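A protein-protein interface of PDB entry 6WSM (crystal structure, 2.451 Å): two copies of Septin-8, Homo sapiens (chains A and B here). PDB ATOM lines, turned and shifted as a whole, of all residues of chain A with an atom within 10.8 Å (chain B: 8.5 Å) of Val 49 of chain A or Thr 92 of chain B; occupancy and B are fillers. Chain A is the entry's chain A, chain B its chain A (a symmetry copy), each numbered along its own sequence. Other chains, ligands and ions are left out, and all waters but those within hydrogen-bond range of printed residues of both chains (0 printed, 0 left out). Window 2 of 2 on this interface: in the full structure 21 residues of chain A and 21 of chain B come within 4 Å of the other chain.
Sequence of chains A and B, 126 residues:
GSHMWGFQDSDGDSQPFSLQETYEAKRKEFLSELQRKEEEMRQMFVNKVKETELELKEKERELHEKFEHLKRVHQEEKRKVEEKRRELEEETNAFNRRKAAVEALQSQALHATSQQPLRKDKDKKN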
ATOM      1  N   MET A  41      11.462  13.565 -24.521  1.00  0.00           N
ATOM      2  CA  MET A  41      12.461  12.694 -25.127  1.00  0.00           C
ATOM      3  C   MET A  41      13.539  13.505 -25.838  1.00  0.00           C
ATOM      4  O   MET A  41      14.726  13.164 -25.769  1.00  0.00           O
ATOM      5  CB  MET A  41      11.794  11.716 -26.095  1.00  0.00           C
ATOM      6  CG  MET A  41      10.915  10.659 -25.439  1.00  0.00           C
ATOM      7  SD  MET A  41      11.799   9.593 -24.290  1.00  0.00           S
ATOM      8  CE  MET A  41      11.243  10.279 -22.733  1.00  0.00           C
ATOM      9  N   ARG A  42      13.147  14.589 -26.513  1.00  0.00           N
ATOM     10  CA  ARG A  42      14.130  15.438 -27.177  1.00  0.00           C
ATOM     11  C   ARG A  42      15.084  16.075 -26.175  1.00  0.00           C
ATOM     12  O   ARG A  42      16.236  16.362 -26.514  1.00  0.00           O
ATOM     13  CB  ARG A  42      13.424  16.514 -28.003  1.00  0.00           C
ATOM     14  N   GLN A  43      14.624  16.302 -24.944  1.00  0.00           N
ATOM     15  CA  GLN A  43      15.489  16.792 -23.880  1.00  0.00           C
ATOM     16  C   GLN A  43      16.207  15.667 -23.147  1.00  0.00           C
ATOM     17  O   GLN A  43      17.269  15.903 -22.561  1.00  0.00           O
ATOM     18  CB  GLN A  43      14.680  17.615 -22.873  1.00  0.00           C
ATOM     19  CG  GLN A  43      13.986  18.828 -23.467  1.00  0.00           C
ATOM     20  CD  GLN A  43      14.958  19.840 -24.045  1.00  0.00           C
ATOM     21  OE1 GLN A  43      16.048  20.049 -23.513  1.00  0.00           O
ATOM     22  NE2 GLN A  43      14.564  20.474 -25.143  1.00  0.00           N
ATOM     23  N   MET A  44      15.651  14.452 -23.161  1.00  0.00           N
ATOM     24  CA  MET A  44      16.316  13.329 -22.507  1.00  0.00           C
ATOM     25  C   MET A  44      17.624  12.983 -23.208  1.00  0.00           C
ATOM     26  O   MET A  44      18.606  12.603 -22.558  1.00  0.00           O
ATOM     27  CB  MET A  44      15.390  12.114 -22.469  1.00  0.00           C
ATOM     28  N   PHE A  45      17.655  13.108 -24.535  1.00  0.00           N
ATOM     29  CA  PHE A  45      18.894  12.866 -25.268  1.00  0.00           C
ATOM     30  C   PHE A  45      19.889  13.998 -25.051  1.00  0.00           C
ATOM     31  O   PHE A  45      21.097  13.756 -24.938  1.00  0.00           O
ATOM     32  CB  PHE A  45      18.596  12.688 -26.757  1.00  0.00           C
ATOM     33  N   VAL A  46      19.401  15.238 -24.994  1.00  0.00           N
ATOM     34  CA  VAL A  46      20.278  16.379 -24.740  1.00  0.00           C
ATOM     35  C   VAL A  46      20.923  16.255 -23.366  1.00  0.00           C
ATOM     36  O   VAL A  46      22.134  16.454 -23.209  1.00  0.00           O
ATOM     37  CB  VAL A  46      19.498  17.697 -24.881  1.00  0.00           C
ATOM     38  CG1 VAL A  46      20.245  18.837 -24.199  1.00  0.00           C
ATOM     39  CG2 VAL A  46      19.263  18.017 -26.349  1.00  0.00           C
ATOM     40  N   ASN A  47      20.123  15.918 -22.352  1.00  0.00           N
ATOM     41  CA  ASN A  47      20.663  15.767 -21.005  1.00  0.00           C
ATOM     42  C   ASN A  47      21.718  14.671 -20.946  1.00  0.00           C
ATOM     43  O   ASN A  47      22.666  14.764 -20.157  1.00  0.00           O
ATOM     44  CB  ASN A  47      19.531  15.484 -20.016  1.00  0.00           C
ATOM     45  CG  ASN A  47      18.582  16.660 -19.866  1.00  0.00           C
ATOM     46  OD1 ASN A  47      18.584  17.583 -20.680  1.00  0.00           O
ATOM     47  ND2 ASN A  47      17.763  16.630 -18.820  1.00  0.00           N
ATOM     48  N   LYS A  48      21.581  13.635 -21.776  1.00  0.00           N
ATOM     49  CA  LYS A  48      22.599  12.594 -21.848  1.00  0.00           C
ATOM     50  C   LYS A  48      23.848  13.062 -22.583  1.00  0.00           C
ATOM     51  O   LYS A  48      24.958  12.639 -22.240  1.00  0.00           O
ATOM     52  CB  LYS A  48      22.029  11.346 -22.524  1.00  0.00           C
ATOM     53  N   VAL A  49      23.696  13.930 -23.587  1.00  0.00           N
ATOM     54  CA  VAL A  49      24.864  14.444 -24.295  1.00  0.00           C
ATOM     55  C   VAL A  49      25.595  15.470 -23.440  1.00  0.00           C
ATOM     56  O   VAL A  49      26.830  15.469 -23.366  1.00  0.00           O
ATOM     57  CB  VAL A  49      24.456  15.033 -25.657  1.00  0.00           C
ATOM     58  CG1 VAL A  49      25.659  15.663 -26.338  1.00  0.00           C
ATOM     59  CG2 VAL A  49      23.858  13.952 -26.541  1.00  0.00           C
ATOM     60  N   LYS A  50      24.848  16.362 -22.782  1.00  0.00           N
ATOM     61  CA  LYS A  50      25.474  17.354 -21.912  1.00  0.00           C
ATOM     62  C   LYS A  50      26.267  16.696 -20.790  1.00  0.00           C
ATOM     63  O   LYS A  50      27.306  17.220 -20.375  1.00  0.00           O
ATOM     64  CB  LYS A  50      24.415  18.291 -21.329  1.00  0.00           C
ATOM     65  CG  LYS A  50      23.624  19.083 -22.360  1.00  0.00           C
ATOM     66  CD  LYS A  50      24.494  20.088 -23.095  1.00  0.00           C
ATOM     67  CE  LYS A  50      23.661  20.942 -24.038  1.00  0.00           C
ATOM     68  NZ  LYS A  50      24.487  21.951 -24.755  1.00  0.00           N
ATOM     69  N   GLU A  51      25.794  15.552 -20.291  1.00  0.00           N
ATOM     70  CA  GLU A  51      26.531  14.837 -19.253  1.00  0.00           C
ATOM     71  C   GLU A  51      27.821  14.246 -19.808  1.00  0.00           C
ATOM     72  O   GLU A  51      28.883  14.350 -19.183  1.00  0.00           O
ATOM     73  CB  GLU A  51      25.652  13.747 -18.641  1.00  0.00           C
ATOM     74  N   THR A  52      27.749  13.620 -20.986  1.00  0.00           N
ATOM     75  CA  THR A  52      28.951  13.060 -21.597  1.00  0.00           C
ATOM     76  C   THR A  52      29.896  14.161 -22.063  1.00  0.00           C
ATOM     77  O   THR A  52      31.121  14.025 -21.946  1.00  0.00           O
ATOM     78  CB  THR A  52      28.578  12.148 -22.766  1.00  0.00           C
ATOM     79  OG1 THR A  52      27.651  11.151 -22.322  1.00  0.00           O
ATOM     80  CG2 THR A  52      29.819  11.461 -23.320  1.00  0.00           C
ATOM     81  N   GLU A  53      29.347  15.258 -22.592  1.00  0.00           N
ATOM     82  CA  GLU A  53      30.183  16.385 -22.995  1.00  0.00           C
ATOM     83  C   GLU A  53      30.969  16.945 -21.819  1.00  0.00           C
ATOM     84  O   GLU A  53      32.091  17.435 -21.996  1.00  0.00           O
ATOM     85  CB  GLU A  53      29.323  17.485 -23.614  1.00  0.00           C
ATOM     86  CG  GLU A  53      29.626  17.779 -25.070  1.00  0.00           C
ATOM     87  CD  GLU A  53      28.761  18.893 -25.622  1.00  0.00           C
ATOM     88  OE1 GLU A  53      29.265  20.026 -25.766  1.00  0.00           O
ATOM     89  OE2 GLU A  53      27.569  18.638 -25.895  1.00  0.00           O
ATOM     90  N   LEU A  54      30.401  16.879 -20.615  1.00  0.00           N
ATOM     91  CA  LEU A  54      31.077  17.406 -19.435  1.00  0.00           C
ATOM     92  C   LEU A  54      32.141  16.443 -18.921  1.00  0.00           C
ATOM     93  O   LEU A  54      33.199  16.881 -18.454  1.00  0.00           O
ATOM     94  CB  LEU A  54      30.052  17.707 -18.343  1.00  0.00           C
ATOM     95  CG  LEU A  54      30.586  18.403 -17.093  1.00  0.00           C
ATOM     96  CD1 LEU A  54      31.207  19.740 -17.461  1.00  0.00           C
ATOM     97  CD2 LEU A  54      29.475  18.584 -16.073  1.00  0.00           C
ATOM     98  N   GLU A  55      31.880  15.135 -18.994  1.00  0.00           N
ATOM     99  CA  GLU A  55      32.863  14.158 -18.539  1.00  0.00           C
ATOM    100  C   GLU A  55      34.137  14.228 -19.372  1.00  0.00           C
ATOM    101  O   GLU A  55      35.245  14.143 -18.831  1.00  0.00           O
ATOM    102  CB  GLU A  55      32.271  12.749 -18.590  1.00  0.00           C
ATOM    103  CG  GLU A  55      31.167  12.489 -17.586  1.00  0.00           C
ATOM    104  CD  GLU A  55      30.727  11.039 -17.579  1.00  0.00           C
ATOM    105  OE1 GLU A  55      31.364  10.221 -18.276  1.00  0.00           O
ATOM    106  OE2 GLU A  55      29.745  10.719 -16.876  1.00  0.00           O
ATOM    107  N   LEU A  56      33.996  14.377 -20.691  1.00  0.00           N
ATOM    108  CA  LEU A  56      35.168  14.528 -21.547  1.00  0.00           C
ATOM    109  C   LEU A  56      35.939  15.794 -21.195  1.00  0.00           C
ATOM    110  O   LEU A  56      37.172  15.821 -21.273  1.00  0.00           O
ATOM    111  CB  LEU A  56      34.745  14.543 -23.016  1.00  0.00           C
ATOM    112  CG  LEU A  56      34.103  13.265 -23.562  1.00  0.00           C
ATOM    113  CD1 LEU A  56      33.577  13.503 -24.968  1.00  0.00           C
ATOM    114  CD2 LEU A  56      35.093  12.108 -23.546  1.00  0.00           C
ATOM    115  N   LYS A  57      35.225  16.853 -20.805  1.00  0.00           N
ATOM    116  CA  LYS A  57      35.891  18.071 -20.352  1.00  0.00           C
ATOM    117  C   LYS A  57      36.671  17.822 -19.066  1.00  0.00           C
ATOM    118  O   LYS A  57      37.793  18.319 -18.906  1.00  0.00           O
ATOM    119  CB  LYS A  57      34.860  19.183 -20.146  1.00  0.00           C
ATOM    120  CG  LYS A  57      35.447  20.558 -19.879  1.00  0.00           C
ATOM    121  CD  LYS A  57      35.938  21.208 -21.161  1.00  0.00           C
ATOM    122  CE  LYS A  57      36.258  22.675 -20.935  1.00  0.00           C
ATOM    123  NZ  LYS A  57      36.634  23.371 -22.196  1.00  0.00           N
ATOM    124  N   GLU A  58      36.091  17.054 -18.140  1.00  0.00           N
ATOM    125  CA  GLU A  58      36.789  16.738 -16.897  1.00  0.00           C
ATOM    126  C   GLU A  58      37.965  15.804 -17.150  1.00  0.00           C
ATOM    127  O   GLU A  58      39.038  15.978 -16.563  1.00  0.00           O
ATOM    128  CB  GLU A  58      35.818  16.121 -15.891  1.00  0.00           C
ATOM    129  N   LYS B  84      35.931  14.444 -29.882  1.00  0.00           N
ATOM    130  CA  LYS B  84      34.709  13.812 -29.395  1.00  0.00           C
ATOM    131  C   LYS B  84      33.731  14.854 -28.872  1.00  0.00           C
ATOM    132  O   LYS B  84      32.517  14.734 -29.071  1.00  0.00           O
ATOM    133  CB  LYS B  84      35.036  12.789 -28.306  1.00  0.00           C
ATOM    134  CG  LYS B  84      35.598  11.477 -28.818  1.00  0.00           C
ATOM    135  CD  LYS B  84      35.677  10.453 -27.696  1.00  0.00           C
ATOM    136  CE  LYS B  84      36.133   9.096 -28.211  1.00  0.00           C
ATOM    137  NZ  LYS B  84      36.132   8.065 -27.133  1.00  0.00           N
ATOM    138  N   ARG B  85      34.244  15.891 -28.201  1.00  0.00           N
ATOM    139  CA  ARG B  85      33.380  16.971 -27.741  1.00  0.00           C
ATOM    140  C   ARG B  85      32.859  17.799 -28.906  1.00  0.00           C
ATOM    141  O   ARG B  85      31.775  18.386 -28.811  1.00  0.00           O
ATOM    142  CB  ARG B  85      34.126  17.857 -26.742  1.00  0.00           C
ATOM    143  CG  ARG B  85      34.462  17.150 -25.441  1.00  0.00           C
ATOM    144  CD  ARG B  85      35.077  18.090 -24.418  1.00  0.00           C
ATOM    145  NE  ARG B  85      34.183  19.188 -24.060  1.00  0.00           N
ATOM    146  CZ  ARG B  85      34.323  20.436 -24.492  1.00  0.00           C
ATOM    147  NH1 ARG B  85      35.328  20.752 -25.299  1.00  0.00           N
ATOM    148  NH2 ARG B  85      33.462  21.370 -24.113  1.00  0.00           N
ATOM    149  N   ARG B  86      33.610  17.861 -30.007  1.00  0.00           N
ATOM    150  CA  ARG B  86      33.081  18.452 -31.229  1.00  0.00           C
ATOM    151  C   ARG B  86      32.133  17.496 -31.942  1.00  0.00           C
ATOM    152  O   ARG B  86      31.232  17.940 -32.661  1.00  0.00           O
ATOM    153  CB  ARG B  86      34.225  18.860 -32.158  1.00  0.00           C
ATOM    154  CG  ARG B  86      33.785  19.690 -33.352  1.00  0.00           C
ATOM    155  CD  ARG B  86      34.968  20.102 -34.210  1.00  0.00           C
ATOM    156  NE  ARG B  86      34.542  20.854 -35.387  1.00  0.00           N
ATOM    157  CZ  ARG B  86      35.370  21.324 -36.314  1.00  0.00           C
ATOM    158  NH1 ARG B  86      36.676  21.123 -36.204  1.00  0.00           N
ATOM    159  NH2 ARG B  86      34.891  21.999 -37.350  1.00  0.00           N
ATOM    160  N   GLU B  87      32.313  16.186 -31.752  1.00  0.00           N
ATOM    161  CA  GLU B  87      31.367  15.208 -32.279  1.00  0.00           C
ATOM    162  C   GLU B  87      30.081  15.149 -31.468  1.00  0.00           C
ATOM    163  O   GLU B  87      29.079  14.612 -31.955  1.00  0.00           O
ATOM    164  CB  GLU B  87      32.009  13.820 -32.325  1.00  0.00           C
ATOM    165  N   LEU B  88      30.088  15.679 -30.245  1.00  0.00           N
ATOM    166  CA  LEU B  88      28.877  15.817 -29.444  1.00  0.00           C
ATOM    167  C   LEU B  88      28.255  17.200 -29.544  1.00  0.00           C
ATOM    168  O   LEU B  88      27.034  17.329 -29.403  1.00  0.00           O
ATOM    169  CB  LEU B  88      29.168  15.508 -27.971  1.00  0.00           C
ATOM    170  CG  LEU B  88      29.454  14.050 -27.610  1.00  0.00           C
ATOM    171  CD1 LEU B  88      29.635  13.888 -26.106  1.00  0.00           C
ATOM    172  CD2 LEU B  88      28.340  13.149 -28.117  1.00  0.00           C
ATOM    173  N   GLU B  89      29.066  18.235 -29.781  1.00  0.00           N
ATOM    174  CA  GLU B  89      28.529  19.581 -29.950  1.00  0.00           C
ATOM    175  C   GLU B  89      27.639  19.672 -31.184  1.00  0.00           C
ATOM    176  O   GLU B  89      26.712  20.489 -31.221  1.00  0.00           O
ATOM    177  CB  GLU B  89      29.676  20.593 -30.035  1.00  0.00           C
ATOM    178  CG  GLU B  89      29.247  22.055 -30.065  1.00  0.00           C
ATOM    179  CD  GLU B  89      29.383  22.682 -31.443  1.00  0.00           C
ATOM    180  OE1 GLU B  89      29.270  21.950 -32.449  1.00  0.00           O
ATOM    181  OE2 GLU B  89      29.610  23.908 -31.518  1.00  0.00           O
ATOM    182  N   GLU B  90      27.897  18.838 -32.194  1.00  0.00           N
ATOM    183  CA  GLU B  90      27.062  18.811 -33.388  1.00  0.00           C
ATOM    184  C   GLU B  90      25.834  17.926 -33.227  1.00  0.00           C
ATOM    185  O   GLU B  90      24.883  18.067 -34.004  1.00  0.00           O
ATOM    186  CB  GLU B  90      27.879  18.340 -34.596  1.00  0.00           C
ATOM    187  CG  GLU B  90      29.132  19.158 -34.873  1.00  0.00           C
ATOM    188  CD  GLU B  90      28.851  20.501 -35.524  1.00  0.00           C
ATOM    189  OE1 GLU B  90      27.704  20.993 -35.449  1.00  0.00           O
ATOM    190  OE2 GLU B  90      29.791  21.067 -36.121  1.00  0.00           O
ATOM    191  N   GLU B  91      25.832  17.015 -32.250  1.00  0.00           N
ATOM    192  CA  GLU B  91      24.643  16.200 -32.011  1.00  0.00           C
ATOM    193  C   GLU B  91      23.560  17.007 -31.306  1.00  0.00           C
ATOM    194  O   GLU B  91      22.367  16.815 -31.565  1.00  0.00           O
ATOM    195  CB  GLU B  91      25.008  14.955 -31.199  1.00  0.00           C
ATOM    196  CG  GLU B  91      25.800  13.921 -31.977  1.00  0.00           C
ATOM    197  CD  GLU B  91      25.995  12.631 -31.203  1.00  0.00           C
ATOM    198  OE1 GLU B  91      25.406  12.497 -30.109  1.00  0.00           O
ATOM    199  OE2 GLU B  91      26.739  11.751 -31.689  1.00  0.00           O
ATOM    200  N   THR B  92      23.957  17.912 -30.408  1.00  0.00           N
ATOM    201  CA  THR B  92      22.989  18.814 -29.793  1.00  0.00           C
ATOM    202  C   THR B  92      22.430  19.795 -30.815  1.00  0.00           C
ATOM    203  O   THR B  92      21.240  20.129 -30.778  1.00  0.00           O
ATOM    204  CB  THR B  92      23.633  19.567 -28.630  1.00  0.00           C
ATOM    205  OG1 THR B  92      24.847  20.183 -29.076  1.00  0.00           O
ATOM    206  CG2 THR B  92      23.943  18.618 -27.487  1.00  0.00           C
ATOM    207  N   ASN B  93      23.276  20.268 -31.734  1.00  0.00           N
ATOM    208  CA  ASN B  93      22.800  21.153 -32.792  1.00  0.00           C
ATOM    209  C   ASN B  93      21.838  20.428 -33.723  1.00  0.00           C
ATOM    210  O   ASN B  93      20.820  20.995 -34.137  1.00  0.00           O
ATOM    211  CB  ASN B  93      23.984  21.712 -33.578  1.00  0.00           C
ATOM    212  CG  ASN B  93      24.882  22.592 -32.731  1.00  0.00           C
ATOM    213  OD1 ASN B  93      24.791  22.591 -31.504  1.00  0.00           O
ATOM    214  ND2 ASN B  93      25.755  23.349 -33.384  1.00  0.00           N
ATOM    215  N   ALA B  94      22.142  19.172 -34.062  1.00  0.00           N
ATOM    216  CA  ALA B  94      21.245  18.395 -34.910  1.00  0.00           C
ATOM    217  C   ALA B  94      19.908  18.157 -34.220  1.00  0.00           C
ATOM    218  O   ALA B  94      18.853  18.191 -34.863  1.00  0.00           O
ATOM    219  CB  ALA B  94      21.898  17.067 -35.291  1.00  0.00           C
ATOM    220  N   PHE B  95      19.932  17.916 -32.907  1.00  0.00           N
ATOM    221  CA  PHE B  95      18.686  17.755 -32.165  1.00  0.00           C
ATOM    222  C   PHE B  95      17.952  19.080 -32.015  1.00  0.00           C
ATOM    223  O   PHE B  95      16.716  19.101 -31.990  1.00  0.00           O
ATOM    224  CB  PHE B  95      18.966  17.140 -30.794  1.00  0.00           C
ATOM    225  N   ASN B  96      18.686  20.192 -31.915  1.00  0.00           N
ATOM    226  CA  ASN B  96      18.047  21.503 -31.869  1.00  0.00           C
ATOM    227  C   ASN B  96      17.413  21.867 -33.206  1.00  0.00           C
ATOM    228  O   ASN B  96      16.399  22.573 -33.236  1.00  0.00           O
ATOM    229  CB  ASN B  96      19.059  22.571 -31.457  1.00  0.00           C
ATOM    230  CG  ASN B  96      19.263  22.633 -29.957  1.00  0.00           C
ATOM    231  OD1 ASN B  96      18.314  22.500 -29.184  1.00  0.00           O
ATOM    232  ND2 ASN B  96      20.506  22.832 -29.538  1.00  0.00           N
ATOM    233  N   ARG B  97      17.998  21.405 -34.314  1.00  0.00           N
ATOM    234  CA  ARG B  97      17.388  21.646 -35.618  1.00  0.00           C
ATOM    235  C   ARG B  97      16.162  20.763 -35.812  1.00  0.00           C
ATOM    236  O   ARG B  97      15.182  21.178 -36.440  1.00  0.00           O
ATOM    237  CB  ARG B  97      18.418  21.421 -36.730  1.00  0.00           C
ATOM    238  CG  ARG B  97      19.457  22.522 -36.811  1.00  0.00           C
ATOM    239  CD  ARG B  97      20.834  21.979 -37.153  1.00  0.00           C
ATOM    240  NE  ARG B  97      21.883  22.951 -36.856  1.00  0.00           N
ATOM    241  CZ  ARG B  97      23.179  22.661 -36.816  1.00  0.00           C
ATOM    242  NH1 ARG B  97      23.588  21.422 -37.051  1.00  0.00           N
ATOM    243  NH2 ARG B  97      24.063  23.608 -36.534  1.00  0.00           N
ATOM    244  N   ARG B  98      16.199  19.535 -35.286  1.00  0.00           N
ATOM    245  CA  ARG B  98      15.013  18.684 -35.328  1.00  0.00           C
ATOM    246  C   ARG B  98      13.886  19.275 -34.491  1.00  0.00           C
ATOM    247  O   ARG B  98      12.710  19.171 -34.860  1.00  0.00           O
ATOM    248  CB  ARG B  98      15.354  17.276 -34.843  1.00  0.00           C
ATOM    249  N   LYS B  99      14.226  19.890 -33.359  1.00  0.00           N
ATOM    250  CA  LYS B  99      13.216  20.550 -32.541  1.00  0.00           C
ATOM    251  C   LYS B  99      12.734  21.838 -33.198  1.00  0.00           C
ATOM    252  O   LYS B  99      11.536  22.142 -33.170  1.00  0.00           O
ATOM    253  CB  LYS B  99      13.778  20.821 -31.146  1.00  0.00           C
ATOM    254  CG  LYS B  99      12.922  21.715 -30.268  1.00  0.00           C
ATOM    255  CD  LYS B  99      13.411  21.667 -28.830  1.00  0.00           C
ATOM    256  CE  LYS B  99      13.204  22.999 -28.122  1.00  0.00           C
ATOM    257  NZ  LYS B  99      13.650  22.922 -26.701  1.00  0.00           N
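O of Gln 43 of chain A lies close to OD1 of Asn 47 of chain A, at 2.8 Å. O of Lys 48 of chain A lies within hydrogen-bond range of OG1 of Thr 52 of chain A (3.1 Å). The side-chain hydroxyl (OG1) of Thr 92 of chain B sits at hydrogen-bond distance from the backbone carbonyl oxygen (O) of Glu 89 of chain B (2.9 Å). OD1 of Asn 93 of chain B sits at hydrogen-bond distance from OG1 of Thr 92 of chain B (3.4 Å). The side-chain amide nitrogen of Asn 96 of chain B is in hydrogen-bond range of the backbone carbonyl oxygen of Thr 92 of chain B.
No position is printed for both chains.
Of the 16 printed residues of chain B, 5 touch a printed residue of chain A. Of the 18 printed residues of chain A, 6 touch a printed residue of chain B. Hydrophobic or aromatic side chains of chain A that line the printed part of chain B: Val 49 and Leu 56. Among the printed residues, no Asp or Glu carboxylate lies within 4 Å of a Lys or Arg side-chain nitrogen of the other chain.
NE2 of Gln 43 of chain A sits close to NZ of Lys 99 of chain B. The guanidinium group of Arg 85 of chain B is in hydrogen-bond range of the backbone carbonyl oxygen of Glu 53 of chain A, 3.4 Å away.
Among the printed residues, merely in contact across the chains: Val 49 of chain A with Leu 88 of chain B, Val 49 of chain A with Thr 92 of chain B, Thr 52 of chain A with Leu 88 of chain B, Glu 53 of chain A with Leu 88 of chain B, Glu 53 of chain A with Thr 92 of chain B, Leu 56 of chain A with Lys 84 of chain B, Leu 56 of chain A with Arg 85 of chain B and Lys 57 of chain A with Arg 85 of chain B.
Of the printed residues of chain B, Gln 43 of chain A touches Lys 99. Of chain B, only Leu 88 (3.7 Å) and Thr 92 (3.6 Å) come within 4 Å of Val 49 of chain A. Printed residues of chain B within 4 Å of Glu 53 of chain A: Arg 85 (3.4 Å), Leu 88 (3.7 Å) and Thr 92 (3.96 Å). Glu 55 of chain A touches none of the printed residues of chain B. Arg 86 of chain B touches none of the printed residues of chain A. Printed residues of chain A within 4 Å of Leu 88 of chain B: Val 49, Thr 52 and Glu 53. No residue of chain A comes within 4 Å of Glu 91 of chain B. Thr 92 of chain B touches just these residues of chain A: Val 49 and Glu 53. Asn 93 of chain B touches none of the printed residues of chain A. No residue of chain A comes within 4 Å of Phe 95 of chain B. No residue of chain A comes within 4 Å of Asn 96 of chain B. The nearest residue of chain B that does not touch Val 49 of chain A is Glu 91 of chain B (4.2 Å).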
